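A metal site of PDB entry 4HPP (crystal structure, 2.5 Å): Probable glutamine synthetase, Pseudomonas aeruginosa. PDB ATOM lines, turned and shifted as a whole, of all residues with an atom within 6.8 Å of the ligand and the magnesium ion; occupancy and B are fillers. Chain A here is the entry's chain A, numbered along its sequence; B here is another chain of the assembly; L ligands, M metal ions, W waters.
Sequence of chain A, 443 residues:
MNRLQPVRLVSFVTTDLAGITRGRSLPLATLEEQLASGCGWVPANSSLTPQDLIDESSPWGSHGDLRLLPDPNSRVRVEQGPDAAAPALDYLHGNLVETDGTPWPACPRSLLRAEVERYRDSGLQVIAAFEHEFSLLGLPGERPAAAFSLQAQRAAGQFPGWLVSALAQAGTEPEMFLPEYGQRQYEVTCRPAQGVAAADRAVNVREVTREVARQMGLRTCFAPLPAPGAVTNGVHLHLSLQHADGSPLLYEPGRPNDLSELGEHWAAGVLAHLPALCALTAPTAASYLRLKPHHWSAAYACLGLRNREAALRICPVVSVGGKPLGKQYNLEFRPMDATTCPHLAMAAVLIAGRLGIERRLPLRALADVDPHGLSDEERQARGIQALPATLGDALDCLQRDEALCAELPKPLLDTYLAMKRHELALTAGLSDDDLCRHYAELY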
ATOM      1  N   GLU A 131     -17.074 -18.083 -18.240  1.00  0.00           N
ATOM      2  CA  GLU A 131     -17.925 -17.452 -19.224  1.00  0.00           C
ATOM      3  C   GLU A 131     -19.321 -17.741 -18.749  1.00  0.00           C
ATOM      4  O   GLU A 131     -19.608 -18.889 -18.376  1.00  0.00           O
ATOM      5  CB  GLU A 131     -17.730 -18.053 -20.622  1.00  0.00           C
ATOM      6  CG  GLU A 131     -16.394 -17.787 -21.346  1.00  0.00           C
ATOM      7  CD  GLU A 131     -16.373 -18.344 -22.790  1.00  0.00           C
ATOM      8  OE1 GLU A 131     -15.444 -17.967 -23.534  1.00  0.00           O
ATOM      9  OE2 GLU A 131     -17.285 -19.131 -23.226  1.00  0.00           O
ATOM     10  N   HIS A 132     -20.173 -16.727 -18.782  1.00  0.00           N
ATOM     11  CA  HIS A 132     -21.487 -16.810 -18.216  1.00  0.00           C
ATOM     12  C   HIS A 132     -22.554 -16.526 -19.221  1.00  0.00           C
ATOM     13  O   HIS A 132     -22.447 -15.550 -19.973  1.00  0.00           O
ATOM     14  CB  HIS A 132     -21.594 -15.832 -17.077  1.00  0.00           C
ATOM     15  CG  HIS A 132     -20.805 -16.244 -15.830  1.00  0.00           C
ATOM     16  ND1 HIS A 132     -19.670 -15.597 -15.438  1.00  0.00           N
ATOM     17  CD2 HIS A 132     -21.087 -17.197 -14.840  1.00  0.00           C
ATOM     18  CE1 HIS A 132     -19.237 -16.135 -14.273  1.00  0.00           C
ATOM     19  NE2 HIS A 132     -20.097 -17.112 -13.925  1.00  0.00           N
ATOM     20  N   GLU A 133     -23.587 -17.393 -19.265  1.00  0.00           N
ATOM     21  CA  GLU A 133     -24.725 -17.122 -20.107  1.00  0.00           C
ATOM     22  C   GLU A 133     -25.983 -16.925 -19.214  1.00  0.00           C
ATOM     23  O   GLU A 133     -26.102 -17.515 -18.130  1.00  0.00           O
ATOM     24  CB  GLU A 133     -24.921 -18.208 -21.140  1.00  0.00           C
ATOM     25  CG  GLU A 133     -23.888 -18.217 -22.264  1.00  0.00           C
ATOM     26  CD  GLU A 133     -23.885 -19.540 -23.026  1.00  0.00           C
ATOM     27  OE1 GLU A 133     -24.525 -20.527 -22.557  1.00  0.00           O
ATOM     28  OE2 GLU A 133     -23.206 -19.603 -24.104  1.00  0.00           O
ATOM     29  N   PHE A 148     -28.030 -14.494 -31.963  1.00  0.00           N
ATOM     30  CA  PHE A 148     -26.706 -13.929 -32.279  1.00  0.00           C
ATOM     31  C   PHE A 148     -26.771 -12.559 -33.003  1.00  0.00           C
ATOM     32  O   PHE A 148     -25.762 -12.073 -33.458  1.00  0.00           O
ATOM     33  CB  PHE A 148     -25.886 -14.941 -33.139  1.00  0.00           C
ATOM     34  CG  PHE A 148     -25.651 -16.313 -32.514  1.00  0.00           C
ATOM     35  CD1 PHE A 148     -25.576 -17.438 -33.326  1.00  0.00           C
ATOM     36  CD2 PHE A 148     -25.447 -16.484 -31.155  1.00  0.00           C
ATOM     37  CE1 PHE A 148     -25.346 -18.714 -32.787  1.00  0.00           C
ATOM     38  CE2 PHE A 148     -25.239 -17.754 -30.619  1.00  0.00           C
ATOM     39  CZ  PHE A 148     -25.193 -18.866 -31.426  1.00  0.00           C
ATOM     40  N   LEU A 178     -22.496 -10.281 -25.829  1.00  0.00           N
ATOM     41  CA  LEU A 178     -23.080 -10.749 -27.086  1.00  0.00           C
ATOM     42  C   LEU A 178     -24.447 -11.390 -26.862  1.00  0.00           C
ATOM     43  O   LEU A 178     -24.648 -12.049 -25.846  1.00  0.00           O
ATOM     44  CB  LEU A 178     -22.102 -11.748 -27.744  1.00  0.00           C
ATOM     45  CG  LEU A 178     -21.531 -12.939 -26.941  1.00  0.00           C
ATOM     46  CD1 LEU A 178     -22.180 -14.251 -27.366  1.00  0.00           C
ATOM     47  CD2 LEU A 178     -20.019 -13.048 -27.077  1.00  0.00           C
ATOM     48  N   GLU A 180     -26.827 -14.474 -27.409  1.00  0.00           N
ATOM     49  CA  GLU A 180     -26.470 -15.881 -27.645  1.00  0.00           C
ATOM     50  C   GLU A 180     -27.620 -16.639 -28.387  1.00  0.00           C
ATOM     51  O   GLU A 180     -28.556 -16.031 -28.946  1.00  0.00           O
ATOM     52  CB  GLU A 180     -26.191 -16.576 -26.310  1.00  0.00           C
ATOM     53  CG  GLU A 180     -24.724 -16.827 -26.021  1.00  0.00           C
ATOM     54  CD  GLU A 180     -24.146 -18.035 -26.732  1.00  0.00           C
ATOM     55  OE1 GLU A 180     -22.947 -18.297 -26.569  1.00  0.00           O
ATOM     56  OE2 GLU A 180     -24.895 -18.733 -27.443  1.00  0.00           O
ATOM     57  N   TYR A 181     -27.576 -17.967 -28.324  1.00  0.00           N
ATOM     58  CA  TYR A 181     -28.430 -18.789 -29.195  1.00  0.00           C
ATOM     59  C   TYR A 181     -29.899 -18.714 -28.779  1.00  0.00           C
ATOM     60  O   TYR A 181     -30.763 -18.537 -29.630  1.00  0.00           O
ATOM     61  CB  TYR A 181     -27.824 -20.240 -29.415  1.00  0.00           C
ATOM     62  CG  TYR A 181     -28.611 -21.106 -30.345  1.00  0.00           C
ATOM     63  CD1 TYR A 181     -28.984 -20.644 -31.620  1.00  0.00           C
ATOM     64  CD2 TYR A 181     -29.011 -22.397 -29.950  1.00  0.00           C
ATOM     65  CE1 TYR A 181     -29.748 -21.428 -32.471  1.00  0.00           C
ATOM     66  CE2 TYR A 181     -29.784 -23.188 -30.792  1.00  0.00           C
ATOM     67  CZ  TYR A 181     -30.154 -22.717 -32.036  1.00  0.00           C
ATOM     68  OH  TYR A 181     -30.908 -23.513 -32.855  1.00  0.00           O
ATOM     69  N   GLN A 185     -31.236 -14.739 -24.600  1.00  0.00           N
ATOM     70  CA  GLN A 185     -29.995 -15.142 -24.021  1.00  0.00           C
ATOM     71  C   GLN A 185     -28.868 -14.167 -24.394  1.00  0.00           C
ATOM     72  O   GLN A 185     -28.729 -13.767 -25.587  1.00  0.00           O
ATOM     73  CB  GLN A 185     -29.645 -16.526 -24.481  1.00  0.00           C
ATOM     74  CG  GLN A 185     -28.588 -17.164 -23.590  1.00  0.00           C
ATOM     75  CD  GLN A 185     -28.177 -18.552 -24.022  1.00  0.00           C
ATOM     76  OE1 GLN A 185     -28.188 -18.892 -25.218  1.00  0.00           O
ATOM     77  NE2 GLN A 185     -27.777 -19.362 -23.039  1.00  0.00           N
ATOM     78  N   GLU A 187     -24.455 -13.282 -23.254  1.00  0.00           N
ATOM     79  CA  GLU A 187     -23.230 -13.754 -22.652  1.00  0.00           C
ATOM     80  C   GLU A 187     -22.276 -12.590 -22.452  1.00  0.00           C
ATOM     81  O   GLU A 187     -22.056 -11.754 -23.333  1.00  0.00           O
ATOM     82  CB  GLU A 187     -22.593 -14.827 -23.514  1.00  0.00           C
ATOM     83  CG  GLU A 187     -21.438 -15.544 -22.808  1.00  0.00           C
ATOM     84  CD  GLU A 187     -20.664 -16.524 -23.707  1.00  0.00           C
ATOM     85  OE1 GLU A 187     -19.650 -17.102 -23.260  1.00  0.00           O
ATOM     86  OE2 GLU A 187     -21.062 -16.735 -24.860  1.00  0.00           O
ATOM     87  N   PRO A 224     -29.522 -23.424 -15.159  1.00  0.00           N
ATOM     88  CA  PRO A 224     -29.087 -24.185 -16.336  1.00  0.00           C
ATOM     89  C   PRO A 224     -30.155 -24.237 -17.425  1.00  0.00           C
ATOM     90  O   PRO A 224     -29.803 -24.094 -18.607  1.00  0.00           O
ATOM     91  CB  PRO A 224     -28.757 -25.600 -15.776  1.00  0.00           C
ATOM     92  CG  PRO A 224     -28.685 -25.463 -14.299  1.00  0.00           C
ATOM     93  CD  PRO A 224     -29.304 -24.138 -13.892  1.00  0.00           C
ATOM     94  N   VAL A 231     -33.059 -23.161 -25.068  1.00  0.00           N
ATOM     95  CA  VAL A 231     -31.595 -23.226 -25.011  1.00  0.00           C
ATOM     96  C   VAL A 231     -31.083 -23.018 -23.579  1.00  0.00           C
ATOM     97  O   VAL A 231     -31.583 -22.161 -22.841  1.00  0.00           O
ATOM     98  CB  VAL A 231     -30.962 -22.156 -25.930  1.00  0.00           C
ATOM     99  CG1 VAL A 231     -29.446 -22.378 -26.070  1.00  0.00           C
ATOM    100  CG2 VAL A 231     -31.678 -22.188 -27.307  1.00  0.00           C
ATOM    101  N   THR A 232     -30.111 -23.841 -23.196  1.00  0.00           N
ATOM    102  CA  THR A 232     -29.615 -23.957 -21.852  1.00  0.00           C
ATOM    103  C   THR A 232     -28.544 -22.866 -21.602  1.00  0.00           C
ATOM    104  O   THR A 232     -27.947 -22.365 -22.557  1.00  0.00           O
ATOM    105  CB  THR A 232     -28.993 -25.362 -21.607  1.00  0.00           C
ATOM    106  OG1 THR A 232     -28.171 -25.750 -22.721  1.00  0.00           O
ATOM    107  CG2 THR A 232     -30.027 -26.419 -21.490  1.00  0.00           C
ATOM    108  N   ASN A 233     -28.309 -22.510 -20.326  1.00  0.00           N
ATOM    109  CA  ASN A 233     -27.366 -21.490 -19.908  1.00  0.00           C
ATOM    110  C   ASN A 233     -26.165 -22.268 -19.324  1.00  0.00           C
ATOM    111  O   ASN A 233     -26.257 -22.871 -18.226  1.00  0.00           O
ATOM    112  CB  ASN A 233     -27.947 -20.511 -18.852  1.00  0.00           C
ATOM    113  CG  ASN A 233     -29.092 -19.585 -19.354  1.00  0.00           C
ATOM    114  OD1 ASN A 233     -28.980 -18.909 -20.404  1.00  0.00           O
ATOM    115  ND2 ASN A 233     -30.211 -19.525 -18.567  1.00  0.00           N
ATOM    116  N   GLY A 234     -25.048 -22.276 -20.054  1.00  0.00           N
ATOM    117  CA  GLY A 234     -23.817 -22.882 -19.576  1.00  0.00           C
ATOM    118  C   GLY A 234     -22.930 -21.903 -18.830  1.00  0.00           C
ATOM    119  O   GLY A 234     -23.203 -20.711 -18.805  1.00  0.00           O
ATOM    120  N   VAL A 235     -21.910 -22.434 -18.173  1.00  0.00           N
ATOM    121  CA  VAL A 235     -20.814 -21.693 -17.609  1.00  0.00           C
ATOM    122  C   VAL A 235     -19.616 -22.481 -18.137  1.00  0.00           C
ATOM    123  O   VAL A 235     -19.608 -23.680 -18.045  1.00  0.00           O
ATOM    124  CB  VAL A 235     -20.825 -21.704 -16.064  1.00  0.00           C
ATOM    125  CG1 VAL A 235     -19.435 -21.352 -15.482  1.00  0.00           C
ATOM    126  CG2 VAL A 235     -21.861 -20.740 -15.503  1.00  0.00           C
ATOM    127  N   HIS A 236     -18.619 -21.809 -18.694  1.00  0.00           N
ATOM    128  CA  HIS A 236     -17.424 -22.503 -19.167  1.00  0.00           C
ATOM    129  C   HIS A 236     -16.229 -21.946 -18.500  1.00  0.00           C
ATOM    130  O   HIS A 236     -16.048 -20.747 -18.404  1.00  0.00           O
ATOM    131  CB  HIS A 236     -17.228 -22.380 -20.682  1.00  0.00           C
ATOM    132  CG  HIS A 236     -18.337 -22.979 -21.497  1.00  0.00           C
ATOM    133  ND1 HIS A 236     -18.611 -22.556 -22.757  1.00  0.00           N
ATOM    134  CD2 HIS A 236     -19.281 -23.983 -21.209  1.00  0.00           C
ATOM    135  CE1 HIS A 236     -19.682 -23.257 -23.248  1.00  0.00           C
ATOM    136  NE2 HIS A 236     -20.096 -24.122 -22.301  1.00  0.00           N
ATOM    137  N   ARG A 290     -29.928 -29.981 -18.440  1.00  0.00           N
ATOM    138  CA  ARG A 290     -28.908 -29.375 -19.324  1.00  0.00           C
ATOM    139  C   ARG A 290     -27.851 -30.405 -19.808  1.00  0.00           C
ATOM    140  O   ARG A 290     -27.565 -30.513 -21.038  1.00  0.00           O
ATOM    141  CB  ARG A 290     -28.254 -28.142 -18.652  1.00  0.00           C
ATOM    142  CG  ARG A 290     -26.924 -27.742 -19.252  1.00  0.00           C
ATOM    143  CD  ARG A 290     -26.401 -26.373 -18.756  1.00  0.00           C
ATOM    144  NE  ARG A 290     -25.215 -26.055 -19.533  1.00  0.00           N
ATOM    145  CZ  ARG A 290     -23.982 -26.534 -19.314  1.00  0.00           C
ATOM    146  NH1 ARG A 290     -22.998 -26.188 -20.140  1.00  0.00           N
ATOM    147  NH2 ARG A 290     -23.704 -27.302 -18.279  1.00  0.00           N
ATOM    148  N   ARG A 308     -17.656 -29.260 -29.778  1.00  0.00           N
ATOM    149  CA  ARG A 308     -18.243 -28.956 -28.478  1.00  0.00           C
ATOM    150  C   ARG A 308     -19.332 -29.966 -28.118  1.00  0.00           C
ATOM    151  O   ARG A 308     -20.393 -29.637 -27.609  1.00  0.00           O
ATOM    152  CB  ARG A 308     -18.811 -27.538 -28.483  1.00  0.00           C
ATOM    153  CG  ARG A 308     -17.799 -26.495 -28.865  1.00  0.00           C
ATOM    154  CD  ARG A 308     -18.480 -25.224 -29.333  1.00  0.00           C
ATOM    155  NE  ARG A 308     -17.506 -24.383 -30.033  1.00  0.00           N
ATOM    156  CZ  ARG A 308     -17.531 -23.062 -30.072  1.00  0.00           C
ATOM    157  NH1 ARG A 308     -18.483 -22.362 -29.446  1.00  0.00           N
ATOM    158  NH2 ARG A 308     -16.582 -22.419 -30.755  1.00  0.00           N
ATOM    159  N   GLU A 332     -10.790 -25.550 -21.785  1.00  0.00           N
ATOM    160  CA  GLU A 332     -12.119 -25.233 -21.413  1.00  0.00           C
ATOM    161  C   GLU A 332     -12.939 -26.475 -20.985  1.00  0.00           C
ATOM    162  O   GLU A 332     -13.190 -27.388 -21.801  1.00  0.00           O
ATOM    163  CB  GLU A 332     -12.756 -24.568 -22.622  1.00  0.00           C
ATOM    164  CG  GLU A 332     -14.242 -24.740 -22.731  1.00  0.00           C
ATOM    165  CD  GLU A 332     -14.889 -23.680 -23.577  1.00  0.00           C
ATOM    166  OE1 GLU A 332     -14.949 -22.498 -23.160  1.00  0.00           O
ATOM    167  OE2 GLU A 332     -15.363 -24.031 -24.664  1.00  0.00           O
ATOM    168  N   ARG A 334     -16.619 -27.828 -19.621  1.00  0.00           N
ATOM    169  CA  ARG A 334     -17.876 -27.397 -20.194  1.00  0.00           C
ATOM    170  C   ARG A 334     -19.095 -27.849 -19.404  1.00  0.00           C
ATOM    171  O   ARG A 334     -20.134 -27.153 -19.467  1.00  0.00           O
ATOM    172  CB  ARG A 334     -17.998 -27.776 -21.676  1.00  0.00           C
ATOM    173  CG  ARG A 334     -16.848 -27.256 -22.498  1.00  0.00           C
ATOM    174  CD  ARG A 334     -16.988 -27.466 -23.991  1.00  0.00           C
ATOM    175  NE  ARG A 334     -17.727 -26.375 -24.629  1.00  0.00           N
ATOM    176  CZ  ARG A 334     -18.938 -26.528 -25.147  1.00  0.00           C
ATOM    177  NH1 ARG A 334     -19.571 -25.489 -25.718  1.00  0.00           N
ATOM    178  NH2 ARG A 334     -19.510 -27.742 -25.092  1.00  0.00           N
ATOM    179  N   MET A 336     -20.572 -27.316 -16.760  1.00  0.00           N
ATOM    180  CA  MET A 336     -20.613 -26.428 -15.618  1.00  0.00           C
ATOM    181  C   MET A 336     -21.721 -25.445 -15.865  1.00  0.00           C
ATOM    182  O   MET A 336     -22.004 -25.145 -17.029  1.00  0.00           O
ATOM    183  CB  MET A 336     -19.281 -25.744 -15.424  1.00  0.00           C
ATOM    184  CG  MET A 336     -19.234 -25.021 -14.100  1.00  0.00           C
ATOM    185  SD  MET A 336     -17.709 -24.083 -13.853  1.00  0.00           S
ATOM    186  CE  MET A 336     -16.545 -25.341 -13.210  1.00  0.00           C
ATOM    187  N   VAL B  42     -18.609 -19.321 -35.100  1.00  0.00           N
ATOM    188  CA  VAL B  42     -18.781 -20.808 -35.150  1.00  0.00           C
ATOM    189  C   VAL B  42     -19.283 -21.107 -36.576  1.00  0.00           C
ATOM    190  O   VAL B  42     -20.242 -20.485 -37.017  1.00  0.00           O
ATOM    191  CB  VAL B  42     -19.756 -21.280 -34.034  1.00  0.00           C
ATOM    192  CG1 VAL B  42     -20.194 -22.728 -34.192  1.00  0.00           C
ATOM    193  CG2 VAL B  42     -19.139 -21.059 -32.650  1.00  0.00           C
HETATM  194  N1  LIG L   1     -25.507 -22.626 -24.067  1.00  0.00           N
HETATM  195  C1  LIG L   1     -24.452 -23.726 -24.144  1.00  0.00           C
HETATM  196  C2  LIG L   1     -24.163 -24.472 -22.826  1.00  0.00           C
HETATM  197  O1  LIG L   1     -25.071 -24.841 -22.080  1.00  0.00           O
HETATM  198  C3  LIG L   1     -23.147 -23.167 -24.695  1.00  0.00           C
HETATM  199  C4  LIG L   1     -23.221 -22.807 -26.157  1.00  0.00           C
HETATM  200  C5  LIG L   1     -22.013 -22.069 -26.609  1.00  0.00           C
HETATM  201  O2  LIG L   1     -21.281 -22.642 -27.432  1.00  0.00           O
HETATM  202  O3  LIG L   1     -21.772 -20.926 -26.139  1.00  0.00           O
HETATM  203  O4  LIG L   1     -23.014 -24.731 -22.447  1.00  0.00           O
HETATM  204 MG    MG M   1     -21.454 -19.183 -25.305  1.00  0.00          MG
HETATM  205  O   HOH W   1     -20.191 -20.119 -22.504  1.00  0.00           O
HETATM  206  O   HOH W   2     -26.555 -21.000 -26.107  1.00  0.00           O
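The guanidinium group (NH1) of Arg 290 is in salt-bridge range of an oxygen (O4) of the ligand, 2.7 Å away. The side-chain hydroxyl of Thr 232 lies within hydrogen-bond range of an oxygen (O1) of the ligand (3.3 Å). An oxygen (O2) of the ligand lies within salt-bridge range of the guanidinium group (NH1) of Arg 308 (3.5 Å). The backbone carbonyl oxygen (O) of Thr 232 is in hydrogen-bond range of a nitrogen (N1) of the ligand (2.9 Å). An oxygen (O1) of the ligand sits at hydrogen-bond distance from the backbone NH (N) of Gly 234 (3.3 Å). NH1 of Arg 334 lies within salt-bridge range of O2 of the ligand (3.7 Å). O4 of the ligand sits at hydrogen-bond distance from NE2 of His 236.
The magnesium ion is bound by an oxygen (O3) of the ligand (2.0 Å), the side-chain carboxylate of Glu 180 (2.1 Å), the side-chain carboxylate of Glu 133 (2.2 Å) and the side-chain carboxylate of Glu 187 (2.5 Å).
Water W2 lies within hydrogen-bond range of N1 of the ligand (2.8 Å), OE1 of Gln 185 (2.8 Å) and OE2 of Glu 180 (3.1 Å). Water W1 lies within hydrogen-bond range of a ring nitrogen (ND1) of His 236 (2.9 Å), the side-chain carboxylate of Glu 131 (3.2 Å) and the side-chain carboxylate of Glu 187 (3.2 Å).
O of Met 336 sits at hydrogen-bond distance from NH2 of Arg 290 (3.0 Å). The guanidinium group (NH1) of Arg 290 lies within hydrogen-bond range of the backbone carbonyl oxygen (O) of Arg 334, 3.1 Å away. O of Leu 178 sits at hydrogen-bond distance from N of Glu 187, at 2.9 Å. The side-chain carboxylate (OE1) of Glu 133 sits at hydrogen-bond distance from the backbone NH (N) of Gly 234 (3.1 Å). The backbone carbonyl oxygen of His 236 is in hydrogen-bond range of the backbone NH of Glu 131, at 2.9 Å. The side-chain amide nitrogen (NE2) of Gln 185 is in hydrogen-bond range of the backbone carbonyl oxygen (O) of Thr 232. The backbone NH (N) of Glu 180 lies within hydrogen-bond range of the backbone carbonyl oxygen (O) of Gln 185. The backbone NH (N) of Asn 233 is in hydrogen-bond range of the backbone carbonyl oxygen (O) of Pro 224, 2.8 Å away.
Residues that only touch the ligand: Asn 233 (3.9 Å). Hydrophobic or aromatic side chains within 4 Å of the ligand: His 236. Nine residues have an atom within 4 Å of the ligand: Glu 133, Glu 180, Thr 232, Asn 233, Gly 234, His 236, Arg 290, Arg 308 and Arg 334.
Within 4 Å of the magnesium ion: Glu 133, Glu 180 and Glu 187.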
